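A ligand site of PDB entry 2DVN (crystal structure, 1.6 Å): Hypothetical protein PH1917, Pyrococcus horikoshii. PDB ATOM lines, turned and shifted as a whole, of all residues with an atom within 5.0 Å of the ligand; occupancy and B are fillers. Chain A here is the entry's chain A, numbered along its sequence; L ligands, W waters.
An oxygen (O1) of the ligand sits close to the side-chain carboxylate (OD1) of Asp 65 (3.3 Å). Glu 36 touches the ligand (OE1 to O3, 3.7 Å). Glu 64 touches the ligand. Ser 81 touches the ligand (CB to O5, 3.4 Å). Ser 82 touches the ligand. Tyr 85 touches the ligand. CZ of Phe 107 touches N4 of the ligand, 3.5 Å away. Phe 140 touches the ligand. Gly 141 touches the ligand (CA to O7, 3.3 Å). Within 4 Å of the ligand: Lys 12, Glu 36, Glu 64, Asp 65, Ser 66, Ser 81, Ser 82, Tyr 85, Phe 107, Phe 140, Gly 141, Tyr 142, Asp 143, Lys 163, His 168 and Arg 169.
NZ of Lys 163 is in salt-bridge range of OD2 of Asp 143 (2.8 Å). O of Asp 143 is in hydrogen-bond range of N of Phe 155, 3.4 Å away. OG of Ser 66 lies within hydrogen-bond range of NH2 of Arg 169 (3.1 Å). The side-chain hydroxyl of Ser 66 sits at hydrogen-bond distance from the side-chain carboxylate of Glu 64, at 2.8 Å. The side-chain amide oxygen (OD1) of Asn 9 lies within hydrogen-bond range of the backbone NH (N) of Lys 12 (3.1 Å). The guanidinium group of Arg 169 is in salt-bridge range of the side-chain carboxylate of Glu 64. OE2 of Glu 15 lies within salt-bridge range of NZ of Lys 163. The side-chain hydroxyl of Tyr 142 lies within hydrogen-bond range of the backbone NH of Tyr 85, at 3.2 Å.
A nitrogen (N3) of the ligand lies within hydrogen-bond range of the side-chain carboxylate (OD1) of Asp 143. The backbone NH of Ser 66 lies within hydrogen-bond range of an oxygen (O2) of the ligand (2.9 Å). O of Ser 66 sits close to O1 of the ligand (2.7 Å). N2 of the ligand lies close to OG of Ser 66. The side-chain amino group (NZ) of Lys 12 lies within salt-bridge range of an oxygen (O2) of the ligand (2.8 Å). NH2 of Arg 169 sits at hydrogen-bond distance from N2 of the ligand, 2.8 Å away. An oxygen (O8) of the ligand is in hydrogen-bond range of the side-chain amino group (NZ) of Lys 163, 2.9 Å away. An oxygen (O8) of the ligand lies close to a ring nitrogen (NE2) of His 168. N of Tyr 142 lies close to N4 of the ligand (3.1 Å).
Water W4 lies within hydrogen-bond range of O3 of the ligand (2.8 Å), OE2 of Glu 36 (3.0 Å) and OD1 of Asp 65 (3.2 Å). Water W7 bridges O7 of the ligand (2.8 Å) and ND2 of Asn 9 (3.1 Å). Water W2 lies within hydrogen-bond range of an oxygen (O3) of the ligand (2.8 Å) and the side-chain hydroxyl (OG) of Ser 82 (3.4 Å). Water W5 lies within hydrogen-bond range of O of Val 79, N of Ser 82, O1 of the ligand and N of Ser 81. Water W6 lies within hydrogen-bond range of ND2 of Asn 9 (2.8 Å) and O4 of the ligand (3.4 Å). Water W3 lies within hydrogen-bond range of OD2 of Asp 65 (2.6 Å), O of Val 79 (2.8 Å) and O1 of the ligand (3.4 Å).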
ATOM      1  N   ASN A   9      -2.147 -22.913  14.455  1.00  0.00           N
ATOM      2  CA  ASN A   9      -1.255 -22.611  15.566  1.00  0.00           C
ATOM      3  C   ASN A   9      -1.633 -21.284  16.221  1.00  0.00           C
ATOM      4  O   ASN A   9      -1.373 -20.206  15.668  1.00  0.00           O
ATOM      5  CB  ASN A   9       0.194 -22.555  15.072  1.00  0.00           C
ATOM      6  CG  ASN A   9       1.205 -22.547  16.197  1.00  0.00           C
ATOM      7  OD1 ASN A   9       1.107 -21.744  17.134  1.00  0.00           O
ATOM      8  ND2 ASN A   9       2.187 -23.429  16.121  1.00  0.00           N
ATOM      9  N   LYS A  12       1.213 -18.669  16.594  1.00  0.00           N
ATOM     10  CA  LYS A  12       1.558 -17.920  15.398  1.00  0.00           C
ATOM     11  C   LYS A  12       0.527 -16.808  15.196  1.00  0.00           C
ATOM     12  O   LYS A  12       0.868 -15.696  14.801  1.00  0.00           O
ATOM     13  CB  LYS A  12       1.548 -18.810  14.152  1.00  0.00           C
ATOM     14  CG  LYS A  12       2.628 -19.877  14.118  1.00  0.00           C
ATOM     15  CD  LYS A  12       2.600 -20.574  12.769  1.00  0.00           C
ATOM     16  CE  LYS A  12       3.533 -21.760  12.701  1.00  0.00           C
ATOM     17  NZ  LYS A  12       3.518 -22.353  11.338  1.00  0.00           N
ATOM     18  N   GLU A  15       1.188 -13.787  17.541  1.00  0.00           N
ATOM     19  CA  GLU A  15       2.379 -13.058  17.138  1.00  0.00           C
ATOM     20  C   GLU A  15       2.159 -12.238  15.866  1.00  0.00           C
ATOM     21  O   GLU A  15       2.573 -11.074  15.795  1.00  0.00           O
ATOM     22  CB  GLU A  15       3.549 -14.027  16.965  1.00  0.00           C
ATOM     23  CG  GLU A  15       4.072 -14.525  18.320  1.00  0.00           C
ATOM     24  CD  GLU A  15       5.044 -15.686  18.225  1.00  0.00           C
ATOM     25  OE1 GLU A  15       5.784 -15.762  17.223  1.00  0.00           O
ATOM     26  OE2 GLU A  15       5.082 -16.517  19.161  1.00  0.00           O
ATOM     27  N   GLU A  36       1.532 -30.423   3.591  1.00  0.00           N
ATOM     28  CA  GLU A  36       2.842 -29.866   3.861  1.00  0.00           C
ATOM     29  C   GLU A  36       3.799 -30.904   3.309  1.00  0.00           C
ATOM     30  O   GLU A  36       4.030 -31.946   3.917  1.00  0.00           O
ATOM     31  CB  GLU A  36       3.022 -29.673   5.367  1.00  0.00           C
ATOM     32  CG  GLU A  36       2.225 -28.486   5.905  1.00  0.00           C
ATOM     33  CD  GLU A  36       2.005 -28.545   7.397  1.00  0.00           C
ATOM     34  OE1 GLU A  36       1.505 -27.550   7.954  1.00  0.00           O
ATOM     35  OE2 GLU A  36       2.321 -29.581   8.011  1.00  0.00           O
ATOM     36  N   LEU A  42      11.826 -24.687   3.647  1.00  0.00           N
ATOM     37  CA  LEU A  42      10.520 -24.261   4.154  1.00  0.00           C
ATOM     38  C   LEU A  42       9.800 -23.570   3.001  1.00  0.00           C
ATOM     39  O   LEU A  42       8.578 -23.645   2.882  1.00  0.00           O
ATOM     40  CB  LEU A  42      10.689 -23.277   5.314  1.00  0.00           C
ATOM     41  CG  LEU A  42      11.338 -23.799   6.600  1.00  0.00           C
ATOM     42  CD1 LEU A  42      11.709 -22.634   7.493  1.00  0.00           C
ATOM     43  CD2 LEU A  42      10.394 -24.751   7.315  1.00  0.00           C
ATOM     44  N   GLU A  64       2.130 -19.826   7.007  1.00  0.00           N
ATOM     45  CA  GLU A  64       3.460 -19.706   7.560  1.00  0.00           C
ATOM     46  C   GLU A  64       4.041 -21.072   7.860  1.00  0.00           C
ATOM     47  O   GLU A  64       3.369 -21.925   8.445  1.00  0.00           O
ATOM     48  CB  GLU A  64       3.426 -18.862   8.840  1.00  0.00           C
ATOM     49  CG  GLU A  64       4.784 -18.278   9.254  1.00  0.00           C
ATOM     50  CD  GLU A  64       5.541 -19.122  10.280  1.00  0.00           C
ATOM     51  OE1 GLU A  64       5.267 -20.330  10.416  1.00  0.00           O
ATOM     52  OE2 GLU A  64       6.438 -18.563  10.936  1.00  0.00           O
ATOM     53  N   ASP A  65       5.287 -21.290   7.437  1.00  0.00           N
ATOM     54  CA  ASP A  65       5.971 -22.549   7.717  1.00  0.00           C
ATOM     55  C   ASP A  65       7.287 -22.142   8.349  1.00  0.00           C
ATOM     56  O   ASP A  65       8.038 -21.346   7.784  1.00  0.00           O
ATOM     57  CB  ASP A  65       6.198 -23.350   6.432  1.00  0.00           C
ATOM     58  CG  ASP A  65       6.343 -24.843   6.707  1.00  0.00           C
ATOM     59  OD1 ASP A  65       5.362 -25.439   7.210  1.00  0.00           O
ATOM     60  OD2 ASP A  65       7.413 -25.409   6.421  1.00  0.00           O
ATOM     61  N   SER A  66       7.574 -22.713   9.516  1.00  0.00           N
ATOM     62  CA  SER A  66       8.783 -22.360  10.232  1.00  0.00           C
ATOM     63  C   SER A  66       9.487 -23.575  10.822  1.00  0.00           C
ATOM     64  O   SER A  66       8.936 -24.674  10.858  1.00  0.00           O
ATOM     65  CB  SER A  66       8.432 -21.367  11.336  1.00  0.00           C
ATOM     66  OG  SER A  66       7.184 -21.697  11.943  1.00  0.00           O
ATOM     67  N   GLY A  67      10.717 -23.378  11.269  1.00  0.00           N
ATOM     68  CA  GLY A  67      11.448 -24.488  11.849  1.00  0.00           C
ATOM     69  C   GLY A  67      12.720 -24.104  12.558  1.00  0.00           C
ATOM     70  O   GLY A  67      13.236 -22.999  12.389  1.00  0.00           O
ATOM     71  N   VAL A  79      12.806 -28.542   8.543  1.00  0.00           N
ATOM     72  CA  VAL A  79      11.502 -28.561   7.900  1.00  0.00           C
ATOM     73  C   VAL A  79      10.522 -29.477   8.643  1.00  0.00           C
ATOM     74  O   VAL A  79       9.312 -29.303   8.558  1.00  0.00           O
ATOM     75  CB  VAL A  79      11.632 -29.044   6.433  1.00  0.00           C
ATOM     76  CG1 VAL A  79      10.269 -29.175   5.784  1.00  0.00           C
ATOM     77  CG2 VAL A  79      12.487 -28.050   5.658  1.00  0.00           C
ATOM     78  N   SER A  81      10.314 -29.848  11.986  1.00  0.00           N
ATOM     79  CA  SER A  81      10.266 -29.436  13.380  1.00  0.00           C
ATOM     80  C   SER A  81       8.965 -29.871  14.071  1.00  0.00           C
ATOM     81  O   SER A  81       8.982 -30.234  15.248  1.00  0.00           O
ATOM     82  CB  SER A  81      10.438 -27.926  13.490  1.00  0.00           C
ATOM     83  OG  SER A  81      11.752 -27.540  13.117  1.00  0.00           O
ATOM     84  N   SER A  82       7.854 -29.831  13.351  1.00  0.00           N
ATOM     85  CA  SER A  82       6.569 -30.219  13.943  1.00  0.00           C
ATOM     86  C   SER A  82       6.534 -31.684  14.354  1.00  0.00           C
ATOM     87  O   SER A  82       6.228 -32.013  15.494  1.00  0.00           O
ATOM     88  CB  SER A  82       5.414 -29.938  12.974  1.00  0.00           C
ATOM     89  OG  SER A  82       4.181 -30.360  13.528  1.00  0.00           O
ATOM     90  N   TYR A  85       8.866 -32.379  17.240  1.00  0.00           N
ATOM     91  CA  TYR A  85       8.353 -31.803  18.472  1.00  0.00           C
ATOM     92  C   TYR A  85       7.272 -32.693  19.095  1.00  0.00           C
ATOM     93  O   TYR A  85       7.245 -32.908  20.309  1.00  0.00           O
ATOM     94  CB  TYR A  85       7.766 -30.405  18.206  1.00  0.00           C
ATOM     95  CG  TYR A  85       7.154 -29.736  19.412  1.00  0.00           C
ATOM     96  CD1 TYR A  85       7.926 -29.443  20.538  1.00  0.00           C
ATOM     97  CD2 TYR A  85       5.798 -29.398  19.435  1.00  0.00           C
ATOM     98  CE1 TYR A  85       7.363 -28.842  21.656  1.00  0.00           C
ATOM     99  CE2 TYR A  85       5.225 -28.788  20.556  1.00  0.00           C
ATOM    100  CZ  TYR A  85       6.021 -28.513  21.660  1.00  0.00           C
ATOM    101  OH  TYR A  85       5.470 -27.930  22.773  1.00  0.00           O
ATOM    102  N   PHE A 107      16.469 -20.185  13.933  1.00  0.00           N
ATOM    103  CA  PHE A 107      15.049 -20.350  13.722  1.00  0.00           C
ATOM    104  C   PHE A 107      14.769 -19.613  12.430  1.00  0.00           C
ATOM    105  O   PHE A 107      15.369 -18.570  12.174  1.00  0.00           O
ATOM    106  CB  PHE A 107      14.258 -19.705  14.863  1.00  0.00           C
ATOM    107  CG  PHE A 107      13.447 -20.681  15.656  1.00  0.00           C
ATOM    108  CD1 PHE A 107      12.492 -21.473  15.025  1.00  0.00           C
ATOM    109  CD2 PHE A 107      13.640 -20.818  17.032  1.00  0.00           C
ATOM    110  CE1 PHE A 107      11.738 -22.391  15.752  1.00  0.00           C
ATOM    111  CE2 PHE A 107      12.886 -21.737  17.758  1.00  0.00           C
ATOM    112  CZ  PHE A 107      11.932 -22.519  17.113  1.00  0.00           C
ATOM    113  N   PHE A 140       5.413 -20.865  22.608  1.00  0.00           N
ATOM    114  CA  PHE A 140       5.008 -22.216  22.270  1.00  0.00           C
ATOM    115  C   PHE A 140       6.155 -23.040  21.688  1.00  0.00           C
ATOM    116  O   PHE A 140       7.274 -22.542  21.541  1.00  0.00           O
ATOM    117  CB  PHE A 140       3.861 -22.149  21.249  1.00  0.00           C
ATOM    118  CG  PHE A 140       4.261 -21.583  19.909  1.00  0.00           C
ATOM    119  CD1 PHE A 140       4.683 -22.417  18.878  1.00  0.00           C
ATOM    120  CD2 PHE A 140       4.193 -20.206  19.678  1.00  0.00           C
ATOM    121  CE1 PHE A 140       5.038 -21.893  17.630  1.00  0.00           C
ATOM    122  CE2 PHE A 140       4.552 -19.671  18.438  1.00  0.00           C
ATOM    123  CZ  PHE A 140       4.968 -20.515  17.413  1.00  0.00           C
ATOM    124  N   GLY A 141       5.876 -24.297  21.365  1.00  0.00           N
ATOM    125  CA  GLY A 141       6.871 -25.168  20.775  1.00  0.00           C
ATOM    126  C   GLY A 141       8.224 -25.210  21.446  1.00  0.00           C
ATOM    127  O   GLY A 141       8.327 -25.444  22.656  1.00  0.00           O
ATOM    128  N   TYR A 142       9.268 -24.977  20.658  1.00  0.00           N
ATOM    129  CA  TYR A 142      10.641 -24.997  21.138  1.00  0.00           C
ATOM    130  C   TYR A 142      11.080 -23.756  21.908  1.00  0.00           C
ATOM    131  O   TYR A 142      12.249 -23.645  22.276  1.00  0.00           O
ATOM    132  CB  TYR A 142      11.602 -25.178  19.951  1.00  0.00           C
ATOM    133  CG  TYR A 142      11.429 -26.466  19.159  1.00  0.00           C
ATOM    134  CD1 TYR A 142      12.157 -27.612  19.477  1.00  0.00           C
ATOM    135  CD2 TYR A 142      10.548 -26.520  18.082  1.00  0.00           C
ATOM    136  CE1 TYR A 142      12.011 -28.790  18.734  1.00  0.00           C
ATOM    137  CE2 TYR A 142      10.395 -27.690  17.330  1.00  0.00           C
ATOM    138  CZ  TYR A 142      11.130 -28.814  17.663  1.00  0.00           C
ATOM    139  OH  TYR A 142      11.008 -29.967  16.925  1.00  0.00           O
ATOM    140  N   ASP A 143      10.163 -22.821  22.160  1.00  0.00           N
ATOM    141  CA  ASP A 143      10.546 -21.604  22.874  1.00  0.00           C
ATOM    142  C   ASP A 143      11.305 -21.810  24.195  1.00  0.00           C
ATOM    143  O   ASP A 143      12.202 -21.047  24.512  1.00  0.00           O
ATOM    144  CB  ASP A 143       9.334 -20.700  23.118  1.00  0.00           C
ATOM    145  CG  ASP A 143       8.920 -19.932  21.864  1.00  0.00           C
ATOM    146  OD1 ASP A 143       9.731 -19.861  20.913  1.00  0.00           O
ATOM    147  OD2 ASP A 143       7.791 -19.396  21.837  1.00  0.00           O
ATOM    148  N   PHE A 155      13.199 -17.834  24.395  1.00  0.00           N
ATOM    149  CA  PHE A 155      11.991 -17.188  23.880  1.00  0.00           C
ATOM    150  C   PHE A 155      10.840 -17.356  24.873  1.00  0.00           C
ATOM    151  O   PHE A 155       9.993 -16.467  24.996  1.00  0.00           O
ATOM    152  CB  PHE A 155      11.567 -17.800  22.540  1.00  0.00           C
ATOM    153  CG  PHE A 155      12.271 -17.245  21.327  1.00  0.00           C
ATOM    154  CD1 PHE A 155      12.791 -15.946  21.323  1.00  0.00           C
ATOM    155  CD2 PHE A 155      12.350 -18.003  20.158  1.00  0.00           C
ATOM    156  CE1 PHE A 155      13.368 -15.419  20.167  1.00  0.00           C
ATOM    157  CE2 PHE A 155      12.927 -17.477  19.002  1.00  0.00           C
ATOM    158  CZ  PHE A 155      13.441 -16.189  19.004  1.00  0.00           C
ATOM    159  N   LYS A 163       9.624 -11.110  22.206  1.00  0.00           N
ATOM    160  CA  LYS A 163       9.908 -12.166  21.246  1.00  0.00           C
ATOM    161  C   LYS A 163       9.809 -11.661  19.814  1.00  0.00           C
ATOM    162  O   LYS A 163      10.706 -11.902  18.991  1.00  0.00           O
ATOM    163  CB  LYS A 163       8.952 -13.356  21.432  1.00  0.00           C
ATOM    164  CG  LYS A 163       9.211 -14.489  20.453  1.00  0.00           C
ATOM    165  CD  LYS A 163       8.210 -15.626  20.634  1.00  0.00           C
ATOM    166  CE  LYS A 163       8.504 -16.733  19.641  1.00  0.00           C
ATOM    167  NZ  LYS A 163       7.454 -17.789  19.626  1.00  0.00           N
ATOM    168  N   HIS A 168      12.523 -14.835  14.431  1.00  0.00           N
ATOM    169  CA  HIS A 168      12.520 -15.126  13.000  1.00  0.00           C
ATOM    170  C   HIS A 168      11.184 -14.680  12.406  1.00  0.00           C
ATOM    171  O   HIS A 168      11.142 -14.197  11.272  1.00  0.00           O
ATOM    172  CB  HIS A 168      12.688 -16.624  12.792  1.00  0.00           C
ATOM    173  CG  HIS A 168      11.770 -17.452  13.637  1.00  0.00           C
ATOM    174  ND1 HIS A 168      11.717 -17.347  15.013  1.00  0.00           N
ATOM    175  CD2 HIS A 168      10.878 -18.419  13.302  1.00  0.00           C
ATOM    176  CE1 HIS A 168      10.836 -18.202  15.488  1.00  0.00           C
ATOM    177  NE2 HIS A 168      10.298 -18.864  14.471  1.00  0.00           N
ATOM    178  N   ARG A 169      10.104 -14.850  13.169  1.00  0.00           N
ATOM    179  CA  ARG A 169       8.770 -14.476  12.715  1.00  0.00           C
ATOM    180  C   ARG A 169       8.626 -12.959  12.659  1.00  0.00           C
ATOM    181  O   ARG A 169       8.027 -12.417  11.728  1.00  0.00           O
ATOM    182  CB  ARG A 169       7.707 -15.101  13.636  1.00  0.00           C
ATOM    183  CG  ARG A 169       6.254 -14.847  13.213  1.00  0.00           C
ATOM    184  CD  ARG A 169       5.289 -15.859  13.845  1.00  0.00           C
ATOM    185  NE  ARG A 169       5.670 -17.211  13.439  1.00  0.00           N
ATOM    186  CZ  ARG A 169       6.276 -18.097  14.210  1.00  0.00           C
ATOM    187  NH1 ARG A 169       6.548 -17.810  15.482  1.00  0.00           N
ATOM    188  NH2 ARG A 169       6.674 -19.248  13.703  1.00  0.00           N
HETATM  189  P1  LIG L   1       5.522 -25.781  10.659  1.00  0.00           P
HETATM  190  O1  LIG L   1       6.828 -26.184  10.043  1.00  0.00           O
HETATM  191  O2  LIG L   1       5.294 -24.320  10.416  1.00  0.00           O
HETATM  192  O3  LIG L   1       4.382 -26.661  10.094  1.00  0.00           O
HETATM  193  O4  LIG L   1       5.559 -25.989  12.151  1.00  0.00           O
HETATM  194  C1  LIG L   1       6.282 -25.542  13.269  1.00  0.00           C
HETATM  195  C2  LIG L   1       7.082 -26.346  14.182  1.00  0.00           C
HETATM  196  O5  LIG L   1       8.241 -25.479  14.468  1.00  0.00           O
HETATM  197  C3  LIG L   1       6.149 -26.452  15.235  1.00  0.00           C
HETATM  198  O6  LIG L   1       6.574 -27.642  15.857  1.00  0.00           O
HETATM  199  C4  LIG L   1       6.518 -25.433  16.247  1.00  0.00           C
HETATM  200  O7  LIG L   1       6.443 -25.811  17.598  1.00  0.00           O
HETATM  201  C5  LIG L   1       7.911 -24.967  15.790  1.00  0.00           C
HETATM  202  N1  LIG L   1       7.976 -23.484  15.757  1.00  0.00           N
HETATM  203  C6  LIG L   1       7.725 -22.582  14.760  1.00  0.00           C
HETATM  204  N2  LIG L   1       7.899 -21.296  15.188  1.00  0.00           N
HETATM  205  C7  LIG L   1       8.264 -21.419  16.483  1.00  0.00           C
HETATM  206  C8  LIG L   1       8.558 -20.415  17.448  1.00  0.00           C
HETATM  207  O8  LIG L   1       8.540 -19.099  17.245  1.00  0.00           O
HETATM  208  N3  LIG L   1       8.921 -20.934  18.750  1.00  0.00           N
HETATM  209  C9  LIG L   1       8.963 -22.311  19.055  1.00  0.00           C
HETATM  210  N4  LIG L   1       8.662 -23.264  18.109  1.00  0.00           N
HETATM  211  C10 LIG L   1       8.320 -22.757  16.878  1.00  0.00           C
HETATM  212  O   HOH W   1       2.794 -24.846   8.334  1.00  0.00           O
HETATM  213  O   HOH W   2       2.547 -28.061  11.646  1.00  0.00           O
HETATM  214  O   HOH W   3       7.390 -27.911   7.124  1.00  0.00           O
HETATM  215  O   HOH W   4       5.071 -28.481   8.148  1.00  0.00           O
HETATM  216  O   HOH W   5       7.507 -29.011  10.605  1.00  0.00           O
HETATM  217  O   HOH W   6       2.764 -24.916  13.777  1.00  0.00           O
HETATM  218  O   HOH W   7       3.708 -25.555  17.819  1.00  0.00           O
